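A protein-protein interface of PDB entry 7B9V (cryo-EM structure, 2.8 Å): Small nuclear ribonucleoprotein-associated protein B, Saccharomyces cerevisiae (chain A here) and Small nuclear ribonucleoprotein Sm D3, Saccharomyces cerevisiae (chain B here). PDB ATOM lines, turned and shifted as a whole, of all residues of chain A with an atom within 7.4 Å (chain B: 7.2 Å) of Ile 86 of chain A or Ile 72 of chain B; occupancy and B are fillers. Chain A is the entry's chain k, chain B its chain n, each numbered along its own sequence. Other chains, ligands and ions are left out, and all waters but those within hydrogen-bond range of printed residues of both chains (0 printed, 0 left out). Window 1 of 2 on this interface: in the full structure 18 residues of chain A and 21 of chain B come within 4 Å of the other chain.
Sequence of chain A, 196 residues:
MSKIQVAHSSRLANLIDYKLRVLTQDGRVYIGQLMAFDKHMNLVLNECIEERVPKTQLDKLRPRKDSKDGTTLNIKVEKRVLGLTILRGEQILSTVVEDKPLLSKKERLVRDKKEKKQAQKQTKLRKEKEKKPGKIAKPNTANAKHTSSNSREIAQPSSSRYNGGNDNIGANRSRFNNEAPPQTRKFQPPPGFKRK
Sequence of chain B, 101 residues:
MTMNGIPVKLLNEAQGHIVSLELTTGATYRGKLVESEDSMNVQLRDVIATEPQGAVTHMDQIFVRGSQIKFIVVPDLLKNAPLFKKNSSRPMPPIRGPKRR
Hydrophobic or aromatic side chains of chain B within 4 Å of the printed part of chain A: Pro 7, Leu 10, Met 40, Phe 71, Val 73 and Val 74. Of the 12 printed residues of chain A, 8 touch a printed residue of chain B. Hydrophobic or aromatic side chains of chain A within 4 Å of the printed part of chain B: Val 44, Leu 82 and Ile 86. Among the printed residues, 18 pairs touch across the chains. Among the printed residues, no Asp or Glu carboxylate lies within 4 Å of a Lys or Arg side-chain nitrogen of the other chain.
Among the printed residues, merely in contact across the chains: Asn 42 of chain A with Pro 7 of chain B, Asn 42 of chain A with Met 40 of chain B, Val 44 of chain A with Pro 7 of chain B, Val 44 of chain A with Leu 10 of chain B, Leu 82 of chain A with Val 73 of chain B, Gly 83 of chain A with Val 73 of chain B, Leu 84 of chain A with Val 74 of chain B, Thr 85 of chain A with Ile 72 of chain B, Thr 85 of chain A with Val 73 of chain B, Ile 86 of chain A with Pro 7 of chain B, Ile 86 of chain A with Leu 10 of chain B, Ile 86 of chain A with Phe 71 of chain B, Ile 86 of chain A with Val 74 of chain B and Arg 88 of chain A with Ile 69 of chain B.
The side-chain carboxylate (OE2) of Glu 22 of chain B is in salt-bridge range of the side-chain amino group (NZ) of Lys 70 of chain B (2.9 Å). The backbone carbonyl oxygen (O) of Ser 20 of chain B lies within hydrogen-bond range of the backbone NH (N) of Val 73 of chain B (2.8 Å). The side-chain amide oxygen (OD1) of Asn 42 of chain A sits at hydrogen-bond distance from the backbone NH (N) of Gly 89 of chain A (2.8 Å). The backbone NH (N) of Glu 22 of chain B is in hydrogen-bond range of the backbone carbonyl oxygen (O) of Phe 71 of chain B, 3.1 Å away. O of Thr 85 of chain A sits at hydrogen-bond distance from N of Leu 45 of chain A, 2.9 Å away.
N of Ile 86 of chain A lies within hydrogen-bond range of O of Ile 72 of chain B. SD of Met 40 of chain B sits at hydrogen-bond distance from NH1 of Arg 88 of chain A (3.3 Å). The backbone carbonyl oxygen (O) of Gly 83 of chain A sits at hydrogen-bond distance from the backbone NH (N) of Val 74 of chain B (3.2 Å). The backbone carbonyl oxygen of Lys 70 of chain B sits at hydrogen-bond distance from the backbone NH of Arg 88 of chain A, at 3.2 Å.
Asn 12 of chain B touches none of the printed residues of chain A. Ser 36 of chain B touches none of the printed residues of chain A. Of the printed residues of chain A, Met 40 of chain B touches Asn 42 (3.9 Å) and Arg 88 (3.3 Å). Printed residues of chain A within 4 Å of Lys 70 of chain B: Arg 88 (3.2 Å). Of the printed residues of chain A, Ile 72 of chain B touches Thr 85 and Ile 86. Printed residues of chain A within 4 Å of Val 74 of chain B: Gly 83, Leu 84 and Ile 86. The nearest residue of chain B that does not touch Ile 86 of chain A is Leu 11 of chain B (4.1 Å). The nearest printed residue of chain A that does not touch Met 40 of chain B is Ile 86 of chain A (4.2 Å).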
ATOM      1  N   ASN A  42      -1.627   0.881  20.249  1.00  0.00           N
ATOM      2  CA  ASN A  42      -0.469   1.543  19.648  1.00  0.00           C
ATOM      3  C   ASN A  42      -0.606   3.036  19.861  1.00  0.00           C
ATOM      4  O   ASN A  42      -1.684   3.593  19.712  1.00  0.00           O
ATOM      5  CB  ASN A  42      -0.386   1.313  18.136  1.00  0.00           C
ATOM      6  CG  ASN A  42       0.043  -0.079  17.746  1.00  0.00           C
ATOM      7  OD1 ASN A  42       0.522  -0.846  18.563  1.00  0.00           O
ATOM      8  ND2 ASN A  42      -0.107  -0.393  16.465  1.00  0.00           N
ATOM      9  N   LEU A  43       0.490   3.669  20.256  1.00  0.00           N
ATOM     10  CA  LEU A  43       0.445   4.965  20.917  1.00  0.00           C
ATOM     11  C   LEU A  43       1.518   5.870  20.331  1.00  0.00           C
ATOM     12  O   LEU A  43       2.706   5.533  20.372  1.00  0.00           O
ATOM     13  CB  LEU A  43       0.623   4.760  22.418  1.00  0.00           C
ATOM     14  CG  LEU A  43      -0.178   5.600  23.388  1.00  0.00           C
ATOM     15  CD1 LEU A  43      -1.621   5.139  23.378  1.00  0.00           C
ATOM     16  CD2 LEU A  43       0.391   5.394  24.748  1.00  0.00           C
ATOM     17  N   VAL A  44       1.103   7.007  19.778  1.00  0.00           N
ATOM     18  CA  VAL A  44       2.020   7.978  19.192  1.00  0.00           C
ATOM     19  C   VAL A  44       2.170   9.182  20.107  1.00  0.00           C
ATOM     20  O   VAL A  44       1.194   9.885  20.400  1.00  0.00           O
ATOM     21  CB  VAL A  44       1.530   8.436  17.814  1.00  0.00           C
ATOM     22  CG1 VAL A  44       2.443   9.505  17.262  1.00  0.00           C
ATOM     23  CG2 VAL A  44       1.451   7.257  16.870  1.00  0.00           C
ATOM     24  N   LEU A  45       3.403   9.415  20.552  1.00  0.00           N
ATOM     25  CA  LEU A  45       3.704  10.451  21.527  1.00  0.00           C
ATOM     26  C   LEU A  45       4.661  11.458  20.914  1.00  0.00           C
ATOM     27  O   LEU A  45       5.795  11.108  20.577  1.00  0.00           O
ATOM     28  CB  LEU A  45       4.318   9.858  22.794  1.00  0.00           C
ATOM     29  CG  LEU A  45       3.537   8.779  23.531  1.00  0.00           C
ATOM     30  CD1 LEU A  45       4.366   8.210  24.660  1.00  0.00           C
ATOM     31  CD2 LEU A  45       2.244   9.335  24.059  1.00  0.00           C
ATOM     32  N   LEU A  82      13.354  11.390  22.849  1.00  0.00           N
ATOM     33  CA  LEU A  82      12.934  10.712  21.640  1.00  0.00           C
ATOM     34  C   LEU A  82      11.935  11.586  20.892  1.00  0.00           C
ATOM     35  O   LEU A  82      11.060  12.197  21.506  1.00  0.00           O
ATOM     36  CB  LEU A  82      12.303   9.377  22.020  1.00  0.00           C
ATOM     37  CG  LEU A  82      13.014   8.395  22.959  1.00  0.00           C
ATOM     38  CD1 LEU A  82      12.113   7.251  23.382  1.00  0.00           C
ATOM     39  CD2 LEU A  82      14.267   7.863  22.291  1.00  0.00           C
ATOM     40  N   GLY A  83      12.045  11.655  19.570  1.00  0.00           N
ATOM     41  CA  GLY A  83      11.136  12.448  18.768  1.00  0.00           C
ATOM     42  C   GLY A  83      10.029  11.632  18.132  1.00  0.00           C
ATOM     43  O   GLY A  83      10.311  10.677  17.403  1.00  0.00           O
ATOM     44  N   LEU A  84       8.765  11.973  18.459  1.00  0.00           N
ATOM     45  CA  LEU A  84       7.549  11.432  17.791  1.00  0.00           C
ATOM     46  C   LEU A  84       7.453   9.895  17.807  1.00  0.00           C
ATOM     47  O   LEU A  84       7.373   9.248  16.755  1.00  0.00           O
ATOM     48  CB  LEU A  84       7.403  12.020  16.383  1.00  0.00           C
ATOM     49  CG  LEU A  84       6.040  11.928  15.660  1.00  0.00           C
ATOM     50  CD1 LEU A  84       5.068  12.733  16.466  1.00  0.00           C
ATOM     51  CD2 LEU A  84       6.128  12.507  14.288  1.00  0.00           C
ATOM     52  N   THR A  85       7.703   9.292  18.971  1.00  0.00           N
ATOM     53  CA  THR A  85       7.717   7.836  19.048  1.00  0.00           C
ATOM     54  C   THR A  85       6.354   7.230  18.752  1.00  0.00           C
ATOM     55  O   THR A  85       5.314   7.749  19.162  1.00  0.00           O
ATOM     56  CB  THR A  85       8.113   7.369  20.445  1.00  0.00           C
ATOM     57  OG1 THR A  85       7.415   8.140  21.425  1.00  0.00           O
ATOM     58  CG2 THR A  85       9.571   7.460  20.621  1.00  0.00           C
ATOM     59  N   ILE A  86       6.383   6.081  18.087  1.00  0.00           N
ATOM     60  CA  ILE A  86       5.275   5.141  18.099  1.00  0.00           C
ATOM     61  C   ILE A  86       5.626   4.065  19.098  1.00  0.00           C
ATOM     62  O   ILE A  86       6.626   3.372  18.924  1.00  0.00           O
ATOM     63  CB  ILE A  86       5.092   4.484  16.724  1.00  0.00           C
ATOM     64  CG1 ILE A  86       4.845   5.506  15.625  1.00  0.00           C
ATOM     65  CG2 ILE A  86       3.967   3.477  16.773  1.00  0.00           C
ATOM     66  CD1 ILE A  86       5.415   5.065  14.290  1.00  0.00           C
ATOM     67  N   LEU A  87       4.795   3.872  20.108  1.00  0.00           N
ATOM     68  CA  LEU A  87       4.946   2.721  20.982  1.00  0.00           C
ATOM     69  C   LEU A  87       4.049   1.590  20.514  1.00  0.00           C
ATOM     70  O   LEU A  87       2.865   1.802  20.241  1.00  0.00           O
ATOM     71  CB  LEU A  87       4.632   3.081  22.434  1.00  0.00           C
ATOM     72  CG  LEU A  87       5.644   3.782  23.344  1.00  0.00           C
ATOM     73  CD1 LEU A  87       5.820   5.228  23.022  1.00  0.00           C
ATOM     74  CD2 LEU A  87       5.191   3.630  24.797  1.00  0.00           C
ATOM     75  N   ARG A  88       4.600   0.388  20.435  1.00  0.00           N
ATOM     76  CA  ARG A  88       3.792  -0.769  20.077  1.00  0.00           C
ATOM     77  C   ARG A  88       2.984  -1.172  21.299  1.00  0.00           C
ATOM     78  O   ARG A  88       3.568  -1.364  22.374  1.00  0.00           O
ATOM     79  CB  ARG A  88       4.656  -1.925  19.600  1.00  0.00           C
ATOM     80  CG  ARG A  88       3.833  -3.085  19.094  1.00  0.00           C
ATOM     81  CD  ARG A  88       4.706  -4.244  18.696  1.00  0.00           C
ATOM     82  NE  ARG A  88       3.924  -5.437  18.389  1.00  0.00           N
ATOM     83  CZ  ARG A  88       3.374  -5.692  17.212  1.00  0.00           C
ATOM     84  NH1 ARG A  88       3.481  -4.843  16.197  1.00  0.00           N
ATOM     85  NH2 ARG A  88       2.691  -6.823  17.051  1.00  0.00           N
ATOM     86  N   GLY A  89       1.646  -1.235  21.136  1.00  0.00           N
ATOM     87  CA  GLY A  89       0.714  -1.374  22.256  1.00  0.00           C
ATOM     88  C   GLY A  89       0.963  -2.565  23.159  1.00  0.00           C
ATOM     89  O   GLY A  89       0.619  -2.532  24.347  1.00  0.00           O
ATOM     90  N   ILE B   6      -4.071   5.680  12.521  1.00  0.00           N
ATOM     91  CA  ILE B   6      -2.969   6.661  12.386  1.00  0.00           C
ATOM     92  C   ILE B   6      -1.599   6.132  12.838  1.00  0.00           C
ATOM     93  O   ILE B   6      -0.629   6.327  12.098  1.00  0.00           O
ATOM     94  CB  ILE B   6      -3.370   7.985  13.049  1.00  0.00           C
ATOM     95  CG1 ILE B   6      -4.379   8.692  12.159  1.00  0.00           C
ATOM     96  CG2 ILE B   6      -2.226   8.975  13.016  1.00  0.00           C
ATOM     97  CD1 ILE B   6      -4.907  10.020  12.689  1.00  0.00           C
ATOM     98  N   PRO B   7      -1.448   5.311  13.986  1.00  0.00           N
ATOM     99  CA  PRO B   7      -0.118   4.770  14.377  1.00  0.00           C
ATOM    100  C   PRO B   7       0.573   3.797  13.405  1.00  0.00           C
ATOM    101  O   PRO B   7       1.646   3.265  13.710  1.00  0.00           O
ATOM    102  CB  PRO B   7      -0.336   4.121  15.747  1.00  0.00           C
ATOM    103  CG  PRO B   7      -1.405   4.860  16.309  1.00  0.00           C
ATOM    104  CD  PRO B   7      -2.333   5.074  15.144  1.00  0.00           C
ATOM    105  N   VAL B   8      -0.041   3.558  12.243  1.00  0.00           N
ATOM    106  CA  VAL B   8       0.513   2.769  11.152  1.00  0.00           C
ATOM    107  C   VAL B   8       0.539   3.566   9.840  1.00  0.00           C
ATOM    108  O   VAL B   8       1.500   3.450   9.071  1.00  0.00           O
ATOM    109  CB  VAL B   8      -0.315   1.454  10.985  1.00  0.00           C
ATOM    110  CG1 VAL B   8       0.034   0.663   9.738  1.00  0.00           C
ATOM    111  CG2 VAL B   8      -0.140   0.559  12.186  1.00  0.00           C
ATOM    112  N   LEU B  10       1.157   6.613   9.929  1.00  0.00           N
ATOM    113  CA  LEU B  10       2.369   7.368  10.258  1.00  0.00           C
ATOM    114  C   LEU B  10       3.613   6.638   9.820  1.00  0.00           C
ATOM    115  O   LEU B  10       4.477   7.232   9.165  1.00  0.00           O
ATOM    116  CB  LEU B  10       2.407   7.677  11.758  1.00  0.00           C
ATOM    117  CG  LEU B  10       3.612   8.441  12.298  1.00  0.00           C
ATOM    118  CD1 LEU B  10       3.670   9.831  11.701  1.00  0.00           C
ATOM    119  CD2 LEU B  10       3.554   8.526  13.801  1.00  0.00           C
ATOM    120  N   LEU B  11       3.740   5.371  10.203  1.00  0.00           N
ATOM    121  CA  LEU B  11       4.911   4.579   9.834  1.00  0.00           C
ATOM    122  C   LEU B  11       4.983   4.312   8.327  1.00  0.00           C
ATOM    123  O   LEU B  11       6.081   4.120   7.788  1.00  0.00           O
ATOM    124  CB  LEU B  11       4.876   3.269  10.621  1.00  0.00           C
ATOM    125  CG  LEU B  11       6.049   2.300  10.500  1.00  0.00           C
ATOM    126  CD1 LEU B  11       7.307   3.000  10.988  1.00  0.00           C
ATOM    127  CD2 LEU B  11       5.743   1.041  11.282  1.00  0.00           C
ATOM    128  N   ASN B  12       3.859   4.406   7.624  1.00  0.00           N
ATOM    129  CA  ASN B  12       3.892   4.419   6.166  1.00  0.00           C
ATOM    130  C   ASN B  12       4.260   5.783   5.594  1.00  0.00           C
ATOM    131  O   ASN B  12       4.752   5.848   4.463  1.00  0.00           O
ATOM    132  CB  ASN B  12       2.554   3.956   5.587  1.00  0.00           C
ATOM    133  CG  ASN B  12       2.411   2.454   5.597  1.00  0.00           C
ATOM    134  OD1 ASN B  12       2.654   1.789   4.592  1.00  0.00           O
ATOM    135  ND2 ASN B  12       2.045   1.911   6.741  1.00  0.00           N
ATOM    136  N   ALA B  14       6.611   7.637   7.096  1.00  0.00           N
ATOM    137  CA  ALA B  14       8.038   7.667   7.447  1.00  0.00           C
ATOM    138  C   ALA B  14       8.996   7.156   6.345  1.00  0.00           C
ATOM    139  O   ALA B  14      10.199   7.058   6.627  1.00  0.00           O
ATOM    140  CB  ALA B  14       8.268   6.885   8.744  1.00  0.00           C
ATOM    141  N   VAL B  19      14.796   6.273  10.666  1.00  0.00           N
ATOM    142  CA  VAL B  19      14.032   5.946  11.866  1.00  0.00           C
ATOM    143  C   VAL B  19      14.903   5.108  12.797  1.00  0.00           C
ATOM    144  O   VAL B  19      15.854   4.452  12.365  1.00  0.00           O
ATOM    145  CB  VAL B  19      12.682   5.223  11.574  1.00  0.00           C
ATOM    146  CG1 VAL B  19      11.797   6.013  10.602  1.00  0.00           C
ATOM    147  CG2 VAL B  19      12.909   3.841  11.031  1.00  0.00           C
ATOM    148  N   SER B  20      14.613   5.181  14.093  1.00  0.00           N
ATOM    149  CA  SER B  20      15.359   4.411  15.079  1.00  0.00           C
ATOM    150  C   SER B  20      14.418   3.448  15.781  1.00  0.00           C
ATOM    151  O   SER B  20      13.372   3.848  16.306  1.00  0.00           O
ATOM    152  CB  SER B  20      16.026   5.315  16.112  1.00  0.00           C
ATOM    153  OG  SER B  20      16.868   4.573  16.978  1.00  0.00           O
ATOM    154  N   LEU B  21      14.781   2.175  15.752  1.00  0.00           N
ATOM    155  CA  LEU B  21      14.012   1.089  16.336  1.00  0.00           C
ATOM    156  C   LEU B  21      14.649   0.632  17.633  1.00  0.00           C
ATOM    157  O   LEU B  21      15.864   0.485  17.696  1.00  0.00           O
ATOM    158  CB  LEU B  21      13.982  -0.087  15.380  1.00  0.00           C
ATOM    159  CG  LEU B  21      12.753  -0.424  14.581  1.00  0.00           C
ATOM    160  CD1 LEU B  21      12.456   0.713  13.611  1.00  0.00           C
ATOM    161  CD2 LEU B  21      13.139  -1.693  13.886  1.00  0.00           C
ATOM    162  N   GLU B  22      13.849   0.379  18.660  1.00  0.00           N
ATOM    163  CA  GLU B  22      14.314  -0.471  19.749  1.00  0.00           C
ATOM    164  C   GLU B  22      13.478  -1.750  19.782  1.00  0.00           C
ATOM    165  O   GLU B  22      12.289  -1.738  19.460  1.00  0.00           O
ATOM    166  CB  GLU B  22      14.306   0.273  21.094  1.00  0.00           C
ATOM    167  CG  GLU B  22      14.901  -0.526  22.264  1.00  0.00           C
ATOM    168  CD  GLU B  22      15.159   0.287  23.501  1.00  0.00           C
ATOM    169  OE1 GLU B  22      15.854   1.320  23.400  1.00  0.00           O
ATOM    170  OE2 GLU B  22      14.704  -0.139  24.587  1.00  0.00           O
ATOM    171  N   LEU B  33      14.328   4.022   6.436  1.00  0.00           N
ATOM    172  CA  LEU B  33      13.166   3.149   6.282  1.00  0.00           C
ATOM    173  C   LEU B  33      12.812   2.899   4.814  1.00  0.00           C
ATOM    174  O   LEU B  33      12.307   3.791   4.128  1.00  0.00           O
ATOM    175  CB  LEU B  33      11.975   3.734   7.034  1.00  0.00           C
ATOM    176  CG  LEU B  33      10.731   2.851   7.067  1.00  0.00           C
ATOM    177  CD1 LEU B  33      10.998   1.726   8.010  1.00  0.00           C
ATOM    178  CD2 LEU B  33       9.529   3.608   7.560  1.00  0.00           C
ATOM    179  N   SER B  36       7.726  -0.457   4.982  1.00  0.00           N
ATOM    180  CA  SER B  36       7.039  -0.825   6.206  1.00  0.00           C
ATOM    181  C   SER B  36       5.700  -1.457   5.862  1.00  0.00           C
ATOM    182  O   SER B  36       5.111  -1.182   4.813  1.00  0.00           O
ATOM    183  CB  SER B  36       6.814   0.390   7.106  1.00  0.00           C
ATOM    184  OG  SER B  36       6.026   1.368   6.448  1.00  0.00           O
ATOM    185  N   MET B  40       3.533  -3.738  11.350  1.00  0.00           N
ATOM    186  CA  MET B  40       4.773  -3.117  11.850  1.00  0.00           C
ATOM    187  C   MET B  40       6.064  -3.867  11.506  1.00  0.00           C
ATOM    188  O   MET B  40       7.069  -3.656  12.178  1.00  0.00           O
ATOM    189  CB  MET B  40       4.723  -2.809  13.356  1.00  0.00           C
ATOM    190  CG  MET B  40       3.580  -1.907  13.754  1.00  0.00           C
ATOM    191  SD  MET B  40       3.529  -1.611  15.527  1.00  0.00           S
ATOM    192  CE  MET B  40       4.939  -0.518  15.720  1.00  0.00           C
ATOM    193  N   ASN B  41       6.098  -4.739  10.495  1.00  0.00           N
ATOM    194  CA  ASN B  41       7.398  -5.147   9.962  1.00  0.00           C
ATOM    195  C   ASN B  41       8.030  -3.948   9.269  1.00  0.00           C
ATOM    196  O   ASN B  41       7.345  -3.153   8.626  1.00  0.00           O
ATOM    197  CB  ASN B  41       7.281  -6.292   8.961  1.00  0.00           C
ATOM    198  CG  ASN B  41       6.613  -7.521   9.532  1.00  0.00           C
ATOM    199  OD1 ASN B  41       6.946  -7.971  10.620  1.00  0.00           O
ATOM    200  ND2 ASN B  41       5.685  -8.081   8.777  1.00  0.00           N
ATOM    201  N   VAL B  42       9.354  -3.834   9.363  1.00  0.00           N
ATOM    202  CA  VAL B  42      10.087  -2.756   8.700  1.00  0.00           C
ATOM    203  C   VAL B  42      11.381  -3.291   8.101  1.00  0.00           C
ATOM    204  O   VAL B  42      11.959  -4.280   8.563  1.00  0.00           O
ATOM    205  CB  VAL B  42      10.406  -1.543   9.629  1.00  0.00           C
ATOM    206  CG1 VAL B  42       9.153  -0.809  10.162  1.00  0.00           C
ATOM    207  CG2 VAL B  42      11.224  -1.986  10.796  1.00  0.00           C
ATOM    208  N   ILE B  69       9.366  -5.283  17.836  1.00  0.00           N
ATOM    209  CA  ILE B  69       9.618  -3.857  17.938  1.00  0.00           C
ATOM    210  C   ILE B  69       8.975  -3.318  19.208  1.00  0.00           C
ATOM    211  O   ILE B  69       7.780  -3.502  19.461  1.00  0.00           O
ATOM    212  CB  ILE B  69       9.134  -3.135  16.676  1.00  0.00           C
ATOM    213  CG1 ILE B  69       9.971  -3.604  15.491  1.00  0.00           C
ATOM    214  CG2 ILE B  69       9.272  -1.668  16.837  1.00  0.00           C
ATOM    215  CD1 ILE B  69       9.592  -3.007  14.174  1.00  0.00           C
ATOM    216  N   LYS B  70       9.788  -2.668  20.021  1.00  0.00           N
ATOM    217  CA  LYS B  70       9.332  -2.021  21.239  1.00  0.00           C
ATOM    218  C   LYS B  70       8.754  -0.652  20.925  1.00  0.00           C
ATOM    219  O   LYS B  70       7.596  -0.371  21.255  1.00  0.00           O
ATOM    220  CB  LYS B  70      10.466  -1.947  22.259  1.00  0.00           C
ATOM    221  CG  LYS B  70       9.994  -1.546  23.648  1.00  0.00           C
ATOM    222  CD  LYS B  70      11.151  -1.219  24.580  1.00  0.00           C
ATOM    223  CE  LYS B  70      12.001  -2.448  24.881  1.00  0.00           C
ATOM    224  NZ  LYS B  70      13.067  -2.124  25.871  1.00  0.00           N
ATOM    225  N   PHE B  71       9.538   0.189  20.254  1.00  0.00           N
ATOM    226  CA  PHE B  71       9.075   1.488  19.801  1.00  0.00           C
ATOM    227  C   PHE B  71       9.865   1.909  18.569  1.00  0.00           C
ATOM    228  O   PHE B  71      10.935   1.369  18.279  1.00  0.00           O
ATOM    229  CB  PHE B  71       9.131   2.539  20.942  1.00  0.00           C
ATOM    230  CG  PHE B  71      10.528   2.827  21.528  1.00  0.00           C
ATOM    231  CD1 PHE B  71      11.502   3.565  20.827  1.00  0.00           C
ATOM    232  CD2 PHE B  71      10.862   2.325  22.766  1.00  0.00           C
ATOM    233  CE1 PHE B  71      12.734   3.801  21.365  1.00  0.00           C
ATOM    234  CE2 PHE B  71      12.114   2.559  23.311  1.00  0.00           C
ATOM    235  CZ  PHE B  71      13.045   3.300  22.606  1.00  0.00           C
ATOM    236  N   ILE B  72       9.314   2.872  17.832  1.00  0.00           N
ATOM    237  CA  ILE B  72       9.942   3.424  16.641  1.00  0.00           C
ATOM    238  C   ILE B  72       9.996   4.936  16.810  1.00  0.00           C
ATOM    239  O   ILE B  72       8.959   5.578  17.004  1.00  0.00           O
ATOM    240  CB  ILE B  72       9.155   3.069  15.362  1.00  0.00           C
ATOM    241  CG1 ILE B  72       9.075   1.566  15.182  1.00  0.00           C
ATOM    242  CG2 ILE B  72       9.785   3.710  14.133  1.00  0.00           C
ATOM    243  CD1 ILE B  72       8.193   1.111  14.080  1.00  0.00           C
ATOM    244  N   VAL B  73      11.195   5.498  16.666  1.00  0.00           N
ATOM    245  CA  VAL B  73      11.417   6.940  16.680  1.00  0.00           C
ATOM    246  C   VAL B  73      11.373   7.455  15.251  1.00  0.00           C
ATOM    247  O   VAL B  73      11.997   6.883  14.353  1.00  0.00           O
ATOM    248  CB  VAL B  73      12.767   7.269  17.347  1.00  0.00           C
ATOM    249  CG1 VAL B  73      13.109   8.768  17.298  1.00  0.00           C
ATOM    250  CG2 VAL B  73      12.803   6.748  18.775  1.00  0.00           C
ATOM    251  N   VAL B  74      10.658   8.558  15.040  1.00  0.00           N
ATOM    252  CA  VAL B  74      10.361   9.064  13.704  1.00  0.00           C
ATOM    253  C   VAL B  74      10.889  10.499  13.624  1.00  0.00           C
ATOM    254  O   VAL B  74      11.122  11.076  14.696  1.00  0.00           O
ATOM    255  CB  VAL B  74       8.824   8.951  13.529  1.00  0.00           C
ATOM    256  CG1 VAL B  74       8.258   9.552  12.311  1.00  0.00           C
ATOM    257  CG2 VAL B  74       8.391   7.475  13.483  1.00  0.00           C
